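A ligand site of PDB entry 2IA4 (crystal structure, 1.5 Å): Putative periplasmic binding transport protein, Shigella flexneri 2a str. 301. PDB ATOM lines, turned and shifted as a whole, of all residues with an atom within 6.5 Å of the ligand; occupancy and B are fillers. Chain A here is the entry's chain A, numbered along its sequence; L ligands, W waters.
The backbone carbonyl oxygen of Ser 90 sits at hydrogen-bond distance from a nitrogen (N1) of the ligand (2.8 Å).
OG of Ser 90 is in hydrogen-bond range of O3 of the ligand (2.7 Å).
The side-chain carboxylate (OD2) of Asp 182 is in salt-bridge range of a nitrogen (N1) of the ligand (2.8 Å).
The guanidinium group of Arg 97 lies within salt-bridge range of an oxygen (O1) of the ligand, at 2.8 Å.
The side-chain hydroxyl of Ser 72 lies within hydrogen-bond range of an oxygen (O2) of the ligand, at 2.8 Å.
The backbone NH (N) of Thr 92 is in hydrogen-bond range of an oxygen (O1) of the ligand (2.8 Å).
The side-chain hydroxyl (OG1) of Thr 92 is in hydrogen-bond range of a nitrogen (N1) of the ligand, 2.8 Å away.
An oxygen (O3) of the ligand is in salt-bridge range of the guanidinium group (NH1) of Arg 24.
An oxygen (O4) of the ligand lies within hydrogen-bond range of the backbone NH (N) of Thr 140 (2.9 Å).
OG1 of Thr 140 lies close to O4 of the ligand (3.5 Å).
An oxygen (O2) of the ligand is in salt-bridge range of the guanidinium group of Arg 75 (2.9 Å).
NE2 of His 164 lies within hydrogen-bond range of O3 of the ligand (2.9 Å).
The side-chain hydroxyl (OG) of Ser 90 sits at hydrogen-bond distance from the guanidinium group (NH1) of Arg 24 (3.4 Å).
The side-chain hydroxyl (OG) of Ser 27 sits at hydrogen-bond distance from the side-chain hydroxyl (OG) of Ser 90, 2.8 Å away.
The side-chain carboxylate (OD2) of Asp 182 lies within hydrogen-bond range of the side-chain hydroxyl (OH) of Tyr 211 (2.6 Å).
The guanidinium group of Arg 24 lies within hydrogen-bond range of the side-chain hydroxyl of Ser 72 (2.8 Å).
The side-chain hydroxyl (OG1) of Thr 92 sits at hydrogen-bond distance from the side-chain carboxylate (OE1) of Glu 209, at 2.6 Å.
The side-chain carboxylate (OD2) of Asp 163 lies within salt-bridge range of the guanidinium group (NH2) of Arg 24 (3.4 Å).
The backbone carbonyl oxygen (O) of Gly 138 sits at hydrogen-bond distance from the guanidinium group (NH2) of Arg 75, at 3.1 Å.
A ring nitrogen (ND1) of His 164 sits at hydrogen-bond distance from the side-chain hydroxyl of Thr 136, at 2.9 Å.
Residues that only touch the ligand: Thr 139, Leu 185, Thr 91, Tyr 211 and Met 181.
Hydrophobic or aromatic side chains that line the ligand: His 164, Met 181, Leu 185 and Tyr 211.
14 residues have an atom within 4 Å of the ligand: Arg 24, Ser 72, Arg 75, Ser 90, Thr 91, Thr 92, Arg 97, Thr 139, Thr 140, His 164, Met 181, Asp 182, Leu 185 and Tyr 211.
Water W1 lies within hydrogen-bond range of OG of Ser 141 (2.6 Å), OG1 of Thr 140 (2.7 Å), OD1 of Asp 182 (2.7 Å) and SD of Met 181 (3.8 Å).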
ATOM      1  N   ARG A  24      -3.997  -3.866 -20.030  1.00  0.00           N
ATOM      2  CA  ARG A  24      -5.437  -3.652 -20.097  1.00  0.00           C
ATOM      3  C   ARG A  24      -6.020  -4.310 -21.341  1.00  0.00           C
ATOM      4  O   ARG A  24      -5.309  -4.650 -22.279  1.00  0.00           O
ATOM      5  CB  ARG A  24      -5.734  -2.142 -20.107  1.00  0.00           C
ATOM      6  CG  ARG A  24      -5.105  -1.395 -18.921  1.00  0.00           C
ATOM      7  CD  ARG A  24      -5.536  -2.020 -17.599  1.00  0.00           C
ATOM      8  NE  ARG A  24      -6.987  -1.923 -17.440  1.00  0.00           N
ATOM      9  CZ  ARG A  24      -7.603  -0.852 -16.948  1.00  0.00           C
ATOM     10  NH1 ARG A  24      -6.904   0.207 -16.547  1.00  0.00           N
ATOM     11  NH2 ARG A  24      -8.939  -0.826 -16.884  1.00  0.00           N
ATOM     12  N   SER A  27      -8.410  -0.195 -22.881  1.00  0.00           N
ATOM     13  CA  SER A  27      -8.010   1.181 -22.603  1.00  0.00           C
ATOM     14  C   SER A  27      -7.419   1.680 -23.905  1.00  0.00           C
ATOM     15  O   SER A  27      -6.207   1.656 -24.102  1.00  0.00           O
ATOM     16  CB  SER A  27      -6.985   1.230 -21.466  1.00  0.00           C
ATOM     17  OG  SER A  27      -7.610   0.949 -20.224  1.00  0.00           O
ATOM     18  N   THR A  71      -7.770  -5.303 -14.405  1.00  0.00           N
ATOM     19  CA  THR A  71      -8.893  -4.374 -14.532  1.00  0.00           C
ATOM     20  C   THR A  71      -8.665  -3.168 -13.628  1.00  0.00           C
ATOM     21  O   THR A  71      -7.784  -3.164 -12.774  1.00  0.00           O
ATOM     22  CB  THR A  71     -10.238  -5.020 -14.111  1.00  0.00           C
ATOM     23  OG1 THR A  71     -10.227  -5.303 -12.713  1.00  0.00           O
ATOM     24  CG2 THR A  71     -10.479  -6.301 -14.897  1.00  0.00           C
ATOM     25  N   SER A  72      -9.481  -2.123 -13.819  1.00  0.00           N
ATOM     26  CA  SER A  72      -9.346  -0.939 -12.986  1.00  0.00           C
ATOM     27  C   SER A  72      -9.612  -1.285 -11.530  1.00  0.00           C
ATOM     28  O   SER A  72      -9.030  -0.700 -10.616  1.00  0.00           O
ATOM     29  CB  SER A  72     -10.324   0.144 -13.451  1.00  0.00           C
ATOM     30  OG  SER A  72      -9.925   0.659 -14.710  1.00  0.00           O
ATOM     31  N   ARG A  75      -6.488  -4.108 -10.208  1.00  0.00           N
ATOM     32  CA  ARG A  75      -5.071  -3.806 -10.412  1.00  0.00           C
ATOM     33  C   ARG A  75      -4.204  -3.690  -9.159  1.00  0.00           C
ATOM     34  O   ARG A  75      -3.105  -4.251  -9.115  1.00  0.00           O
ATOM     35  CB  ARG A  75      -4.897  -2.556 -11.274  1.00  0.00           C
ATOM     36  CG  ARG A  75      -5.489  -1.299 -10.700  1.00  0.00           C
ATOM     37  CD  ARG A  75      -5.430  -0.135 -11.679  1.00  0.00           C
ATOM     38  NE  ARG A  75      -6.446   0.845 -11.331  1.00  0.00           N
ATOM     39  CZ  ARG A  75      -6.940   1.760 -12.151  1.00  0.00           C
ATOM     40  NH1 ARG A  75      -6.489   1.855 -13.396  1.00  0.00           N
ATOM     41  NH2 ARG A  75      -7.918   2.552 -11.740  1.00  0.00           N
ATOM     42  N   GLY A  89      -0.695   1.645 -18.714  1.00  0.00           N
ATOM     43  CA  GLY A  89      -1.958   1.688 -19.416  1.00  0.00           C
ATOM     44  C   GLY A  89      -2.666   3.000 -19.233  1.00  0.00           C
ATOM     45  O   GLY A  89      -2.290   3.997 -19.840  1.00  0.00           O
ATOM     46  N   SER A  90      -3.697   3.014 -18.394  1.00  0.00           N
ATOM     47  CA  SER A  90      -4.469   4.223 -18.149  1.00  0.00           C
ATOM     48  C   SER A  90      -4.748   4.425 -16.653  1.00  0.00           C
ATOM     49  O   SER A  90      -5.817   4.900 -16.278  1.00  0.00           O
ATOM     50  CB  SER A  90      -5.790   4.136 -18.920  1.00  0.00           C
ATOM     51  OG  SER A  90      -6.503   2.947 -18.595  1.00  0.00           O
ATOM     52  N   THR A  91      -3.771   4.095 -15.815  1.00  0.00           N
ATOM     53  CA  THR A  91      -3.934   4.257 -14.375  1.00  0.00           C
ATOM     54  C   THR A  91      -3.473   5.625 -13.911  1.00  0.00           C
ATOM     55  O   THR A  91      -2.345   6.043 -14.184  1.00  0.00           O
ATOM     56  CB  THR A  91      -3.134   3.185 -13.603  1.00  0.00           C
ATOM     57  OG1 THR A  91      -3.554   1.894 -14.027  1.00  0.00           O
ATOM     58  CG2 THR A  91      -3.351   3.334 -12.103  1.00  0.00           C
ATOM     59  N   THR A  92      -4.368   6.317 -13.222  1.00  0.00           N
ATOM     60  CA  THR A  92      -4.088   7.643 -12.693  1.00  0.00           C
ATOM     61  C   THR A  92      -3.184   7.567 -11.477  1.00  0.00           C
ATOM     62  O   THR A  92      -3.395   6.743 -10.577  1.00  0.00           O
ATOM     63  CB  THR A  92      -5.368   8.366 -12.290  1.00  0.00           C
ATOM     64  OG1 THR A  92      -6.090   8.721 -13.470  1.00  0.00           O
ATOM     65  CG2 THR A  92      -5.064   9.628 -11.475  1.00  0.00           C
ATOM     66  N   ASN A  93      -2.186   8.426 -11.466  1.00  0.00           N
ATOM     67  CA  ASN A  93      -1.263   8.528 -10.355  1.00  0.00           C
ATOM     68  C   ASN A  93      -1.820   9.607  -9.431  1.00  0.00           C
ATOM     69  O   ASN A  93      -1.958  10.767  -9.827  1.00  0.00           O
ATOM     70  CB  ASN A  93       0.123   8.932 -10.876  1.00  0.00           C
ATOM     71  CG  ASN A  93       1.063   9.418  -9.773  1.00  0.00           C
ATOM     72  OD1 ASN A  93       0.772   9.316  -8.586  1.00  0.00           O
ATOM     73  ND2 ASN A  93       2.216   9.952 -10.181  1.00  0.00           N
ATOM     74  N   ARG A  97      -3.416   6.594  -4.005  1.00  0.00           N
ATOM     75  CA  ARG A  97      -2.874   5.356  -4.528  1.00  0.00           C
ATOM     76  C   ARG A  97      -1.382   5.200  -4.223  1.00  0.00           C
ATOM     77  O   ARG A  97      -0.867   4.084  -4.204  1.00  0.00           O
ATOM     78  CB  ARG A  97      -3.113   5.269  -6.034  1.00  0.00           C
ATOM     79  CG  ARG A  97      -4.589   5.133  -6.369  1.00  0.00           C
ATOM     80  CD  ARG A  97      -4.827   5.176  -7.858  1.00  0.00           C
ATOM     81  NE  ARG A  97      -6.245   4.954  -8.165  1.00  0.00           N
ATOM     82  CZ  ARG A  97      -6.741   4.959  -9.393  1.00  0.00           C
ATOM     83  NH1 ARG A  97      -5.950   5.168 -10.436  1.00  0.00           N
ATOM     84  NH2 ARG A  97      -8.045   4.742  -9.572  1.00  0.00           N
ATOM     85  N   VAL A 110      -5.183  13.424 -18.858  1.00  0.00           N
ATOM     86  CA  VAL A 110      -6.580  13.384 -19.298  1.00  0.00           C
ATOM     87  C   VAL A 110      -7.511  14.230 -18.442  1.00  0.00           C
ATOM     88  O   VAL A 110      -7.165  14.658 -17.338  1.00  0.00           O
ATOM     89  CB  VAL A 110      -7.131  11.938 -19.277  1.00  0.00           C
ATOM     90  CG1 VAL A 110      -6.278  11.031 -20.143  1.00  0.00           C
ATOM     91  CG2 VAL A 110      -7.186  11.431 -17.837  1.00  0.00           C
ATOM     92  N   THR A 112     -11.613  14.199 -17.064  1.00  0.00           N
ATOM     93  CA  THR A 112     -12.771  13.316 -16.943  1.00  0.00           C
ATOM     94  C   THR A 112     -14.048  13.996 -17.430  1.00  0.00           C
ATOM     95  O   THR A 112     -14.506  14.978 -16.856  1.00  0.00           O
ATOM     96  CB  THR A 112     -12.933  12.825 -15.478  1.00  0.00           C
ATOM     97  OG1 THR A 112     -12.891  13.944 -14.579  1.00  0.00           O
ATOM     98  CG2 THR A 112     -11.799  11.866 -15.133  1.00  0.00           C
ATOM     99  N   THR A 136     -16.900   2.941 -15.113  1.00  0.00           N
ATOM    100  CA  THR A 136     -16.136   1.706 -14.905  1.00  0.00           C
ATOM    101  C   THR A 136     -15.745   1.541 -13.438  1.00  0.00           C
ATOM    102  O   THR A 136     -15.259   2.463 -12.793  1.00  0.00           O
ATOM    103  CB  THR A 136     -14.869   1.708 -15.788  1.00  0.00           C
ATOM    104  OG1 THR A 136     -15.245   1.823 -17.161  1.00  0.00           O
ATOM    105  CG2 THR A 136     -14.088   0.406 -15.588  1.00  0.00           C
ATOM    106  N   SER A 137     -15.965   0.334 -12.915  1.00  0.00           N
ATOM    107  CA  SER A 137     -15.653   0.041 -11.525  1.00  0.00           C
ATOM    108  C   SER A 137     -14.175   0.217 -11.207  1.00  0.00           C
ATOM    109  O   SER A 137     -13.312  -0.163 -12.000  1.00  0.00           O
ATOM    110  CB  SER A 137     -16.054  -1.398 -11.190  1.00  0.00           C
ATOM    111  OG  SER A 137     -17.438  -1.615 -11.402  1.00  0.00           O
ATOM    112  N   GLY A 138     -13.896   0.790 -10.038  1.00  0.00           N
ATOM    113  CA  GLY A 138     -12.531   0.969  -9.596  1.00  0.00           C
ATOM    114  C   GLY A 138     -11.766   2.148 -10.169  1.00  0.00           C
ATOM    115  O   GLY A 138     -10.539   2.220 -10.025  1.00  0.00           O
ATOM    116  N   THR A 139     -12.471   3.073 -10.806  1.00  0.00           N
ATOM    117  CA  THR A 139     -11.826   4.241 -11.399  1.00  0.00           C
ATOM    118  C   THR A 139     -12.028   5.518 -10.592  1.00  0.00           C
ATOM    119  O   THR A 139     -12.900   5.595  -9.723  1.00  0.00           O
ATOM    120  CB  THR A 139     -12.361   4.528 -12.815  1.00  0.00           C
ATOM    121  OG1 THR A 139     -13.761   4.793 -12.746  1.00  0.00           O
ATOM    122  CG2 THR A 139     -12.112   3.356 -13.743  1.00  0.00           C
ATOM    123  N   THR A 140     -11.214   6.524 -10.892  1.00  0.00           N
ATOM    124  CA  THR A 140     -11.334   7.808 -10.236  1.00  0.00           C
ATOM    125  C   THR A 140     -12.670   8.441 -10.624  1.00  0.00           C
ATOM    126  O   THR A 140     -13.257   9.201  -9.849  1.00  0.00           O
ATOM    127  CB  THR A 140     -10.179   8.743 -10.629  1.00  0.00           C
ATOM    128  OG1 THR A 140      -9.950   8.644 -12.037  1.00  0.00           O
ATOM    129  CG2 THR A 140      -8.899   8.378  -9.882  1.00  0.00           C
ATOM    130  N   SER A 141     -13.162   8.143 -11.826  1.00  0.00           N
ATOM    131  CA  SER A 141     -14.444   8.690 -12.251  1.00  0.00           C
ATOM    132  C   SER A 141     -15.573   8.126 -11.403  1.00  0.00           C
ATOM    133  O   SER A 141     -16.518   8.839 -11.064  1.00  0.00           O
ATOM    134  CB  SER A 141     -14.711   8.397 -13.734  1.00  0.00           C
ATOM    135  OG  SER A 141     -13.988   9.297 -14.565  1.00  0.00           O
ATOM    136  N   ASP A 163     -15.267  -3.044 -17.254  1.00  0.00           N
ATOM    137  CA  ASP A 163     -14.199  -2.423 -18.018  1.00  0.00           C
ATOM    138  C   ASP A 163     -14.788  -1.373 -18.940  1.00  0.00           C
ATOM    139  O   ASP A 163     -16.013  -1.269 -19.076  1.00  0.00           O
ATOM    140  CB  ASP A 163     -13.421  -3.480 -18.815  1.00  0.00           C
ATOM    141  CG  ASP A 163     -11.936  -3.131 -18.974  1.00  0.00           C
ATOM    142  OD1 ASP A 163     -11.161  -4.019 -19.400  1.00  0.00           O
ATOM    143  OD2 ASP A 163     -11.549  -1.971 -18.689  1.00  0.00           O
ATOM    144  N   HIS A 164     -13.943  -0.577 -19.572  1.00  0.00           N
ATOM    145  CA  HIS A 164     -14.413   0.514 -20.419  1.00  0.00           C
ATOM    146  C   HIS A 164     -15.311   0.140 -21.585  1.00  0.00           C
ATOM    147  O   HIS A 164     -16.252   0.863 -21.894  1.00  0.00           O
ATOM    148  CB  HIS A 164     -13.216   1.337 -20.896  1.00  0.00           C
ATOM    149  CG  HIS A 164     -12.312   1.746 -19.769  1.00  0.00           C
ATOM    150  ND1 HIS A 164     -12.793   2.265 -18.591  1.00  0.00           N
ATOM    151  CD2 HIS A 164     -10.965   1.647 -19.620  1.00  0.00           C
ATOM    152  CE1 HIS A 164     -11.783   2.486 -17.768  1.00  0.00           C
ATOM    153  NE2 HIS A 164     -10.669   2.112 -18.363  1.00  0.00           N
ATOM    154  N   MET A 181     -15.921   9.156 -18.010  1.00  0.00           N
ATOM    155  CA  MET A 181     -14.579   8.577 -18.007  1.00  0.00           C
ATOM    156  C   MET A 181     -13.555   9.527 -18.611  1.00  0.00           C
ATOM    157  O   MET A 181     -13.925  10.546 -19.199  1.00  0.00           O
ATOM    158  CB  MET A 181     -14.586   7.264 -18.801  1.00  0.00           C
ATOM    159  CG  MET A 181     -13.316   6.422 -18.691  1.00  0.00           C
ATOM    160  SD  MET A 181     -12.754   6.065 -16.870  1.00  0.00           S
ATOM    161  CE  MET A 181     -14.394   5.235 -16.215  1.00  0.00           C
ATOM    162  N   ASP A 182     -12.276   9.212 -18.428  1.00  0.00           N
ATOM    163  CA  ASP A 182     -11.179  10.006 -18.984  1.00  0.00           C
ATOM    164  C   ASP A 182     -11.521  10.271 -20.451  1.00  0.00           C
ATOM    165  O   ASP A 182     -11.863   9.332 -21.176  1.00  0.00           O
ATOM    166  CB  ASP A 182      -9.874   9.207 -18.925  1.00  0.00           C
ATOM    167  CG  ASP A 182      -9.529   8.717 -17.530  1.00  0.00           C
ATOM    168  OD1 ASP A 182     -10.272   9.010 -16.564  1.00  0.00           O
ATOM    169  OD2 ASP A 182      -8.483   8.039 -17.396  1.00  0.00           O
ATOM    170  N   LEU A 185     -10.040   7.945 -23.144  1.00  0.00           N
ATOM    171  CA  LEU A 185     -10.625   6.610 -23.139  1.00  0.00           C
ATOM    172  C   LEU A 185     -12.005   6.612 -23.787  1.00  0.00           C
ATOM    173  O   LEU A 185     -12.388   5.650 -24.453  1.00  0.00           O
ATOM    174  CB  LEU A 185     -10.710   6.061 -21.714  1.00  0.00           C
ATOM    175  CG  LEU A 185      -9.362   5.776 -21.024  1.00  0.00           C
ATOM    176  CD1 LEU A 185      -9.612   5.320 -19.595  1.00  0.00           C
ATOM    177  CD2 LEU A 185      -8.587   4.732 -21.805  1.00  0.00           C
ATOM    178  N   GLU A 209      -6.113  14.505 -14.705  1.00  0.00           N
ATOM    179  CA  GLU A 209      -5.344  13.406 -14.137  1.00  0.00           C
ATOM    180  C   GLU A 209      -4.150  12.938 -14.962  1.00  0.00           C
ATOM    181  O   GLU A 209      -4.197  12.907 -16.181  1.00  0.00           O
ATOM    182  CB  GLU A 209      -6.302  12.232 -13.872  1.00  0.00           C
ATOM    183  CG  GLU A 209      -7.360  12.576 -12.843  1.00  0.00           C
ATOM    184  CD  GLU A 209      -8.395  11.486 -12.635  1.00  0.00           C
ATOM    185  OE1 GLU A 209      -8.072  10.300 -12.855  1.00  0.00           O
ATOM    186  OE2 GLU A 209      -9.536  11.817 -12.232  1.00  0.00           O
ATOM    187  N   ALA A 210      -3.081  12.565 -14.261  1.00  0.00           N
ATOM    188  CA  ALA A 210      -1.870  12.097 -14.913  1.00  0.00           C
ATOM    189  C   ALA A 210      -1.755  10.573 -14.900  1.00  0.00           C
ATOM    190  O   ALA A 210      -1.947   9.941 -13.861  1.00  0.00           O
ATOM    191  CB  ALA A 210      -0.638  12.708 -14.245  1.00  0.00           C
ATOM    192  N   TYR A 211      -1.467   9.993 -16.066  1.00  0.00           N
ATOM    193  CA  TYR A 211      -1.277   8.549 -16.210  1.00  0.00           C
ATOM    194  C   TYR A 211       0.189   8.243 -15.925  1.00  0.00           C
ATOM    195  O   TYR A 211       1.074   8.973 -16.356  1.00  0.00           O
ATOM    196  CB  TYR A 211      -1.539   8.082 -17.636  1.00  0.00           C
ATOM    197  CG  TYR A 211      -2.966   7.947 -18.075  1.00  0.00           C
ATOM    198  CD1 TYR A 211      -4.034   8.311 -17.244  1.00  0.00           C
ATOM    199  CD2 TYR A 211      -3.258   7.470 -19.347  1.00  0.00           C
ATOM    200  CE1 TYR A 211      -5.359   8.178 -17.685  1.00  0.00           C
ATOM    201  CE2 TYR A 211      -4.562   7.335 -19.795  1.00  0.00           C
ATOM    202  CZ  TYR A 211      -5.597   7.693 -18.963  1.00  0.00           C
ATOM    203  OH  TYR A 211      -6.890   7.562 -19.424  1.00  0.00           O
HETATM  204  N1  LIG L   1      -7.422   6.863 -15.120  1.00  0.00           N
HETATM  205  C1  LIG L   1      -8.589   6.472 -14.274  1.00  0.00           C
HETATM  206  C2  LIG L   1      -8.168   5.588 -13.110  1.00  0.00           C
HETATM  207  O1  LIG L   1      -6.973   5.232 -13.057  1.00  0.00           O
HETATM  208  C3  LIG L   1      -9.650   5.761 -15.132  1.00  0.00           C
HETATM  209  C4  LIG L   1      -9.129   4.857 -16.249  1.00  0.00           C
HETATM  210  C5  LIG L   1      -8.709   3.468 -15.777  1.00  0.00           C
HETATM  211  O2  LIG L   1      -8.753   3.215 -14.555  1.00  0.00           O
HETATM  212  O3  LIG L   1      -8.347   2.643 -16.635  1.00  0.00           O
HETATM  213  O4  LIG L   1      -9.034   5.274 -12.262  1.00  0.00           O
HETATM  214  O   HOH W   1     -11.528   8.425 -14.205  1.00  0.00           O
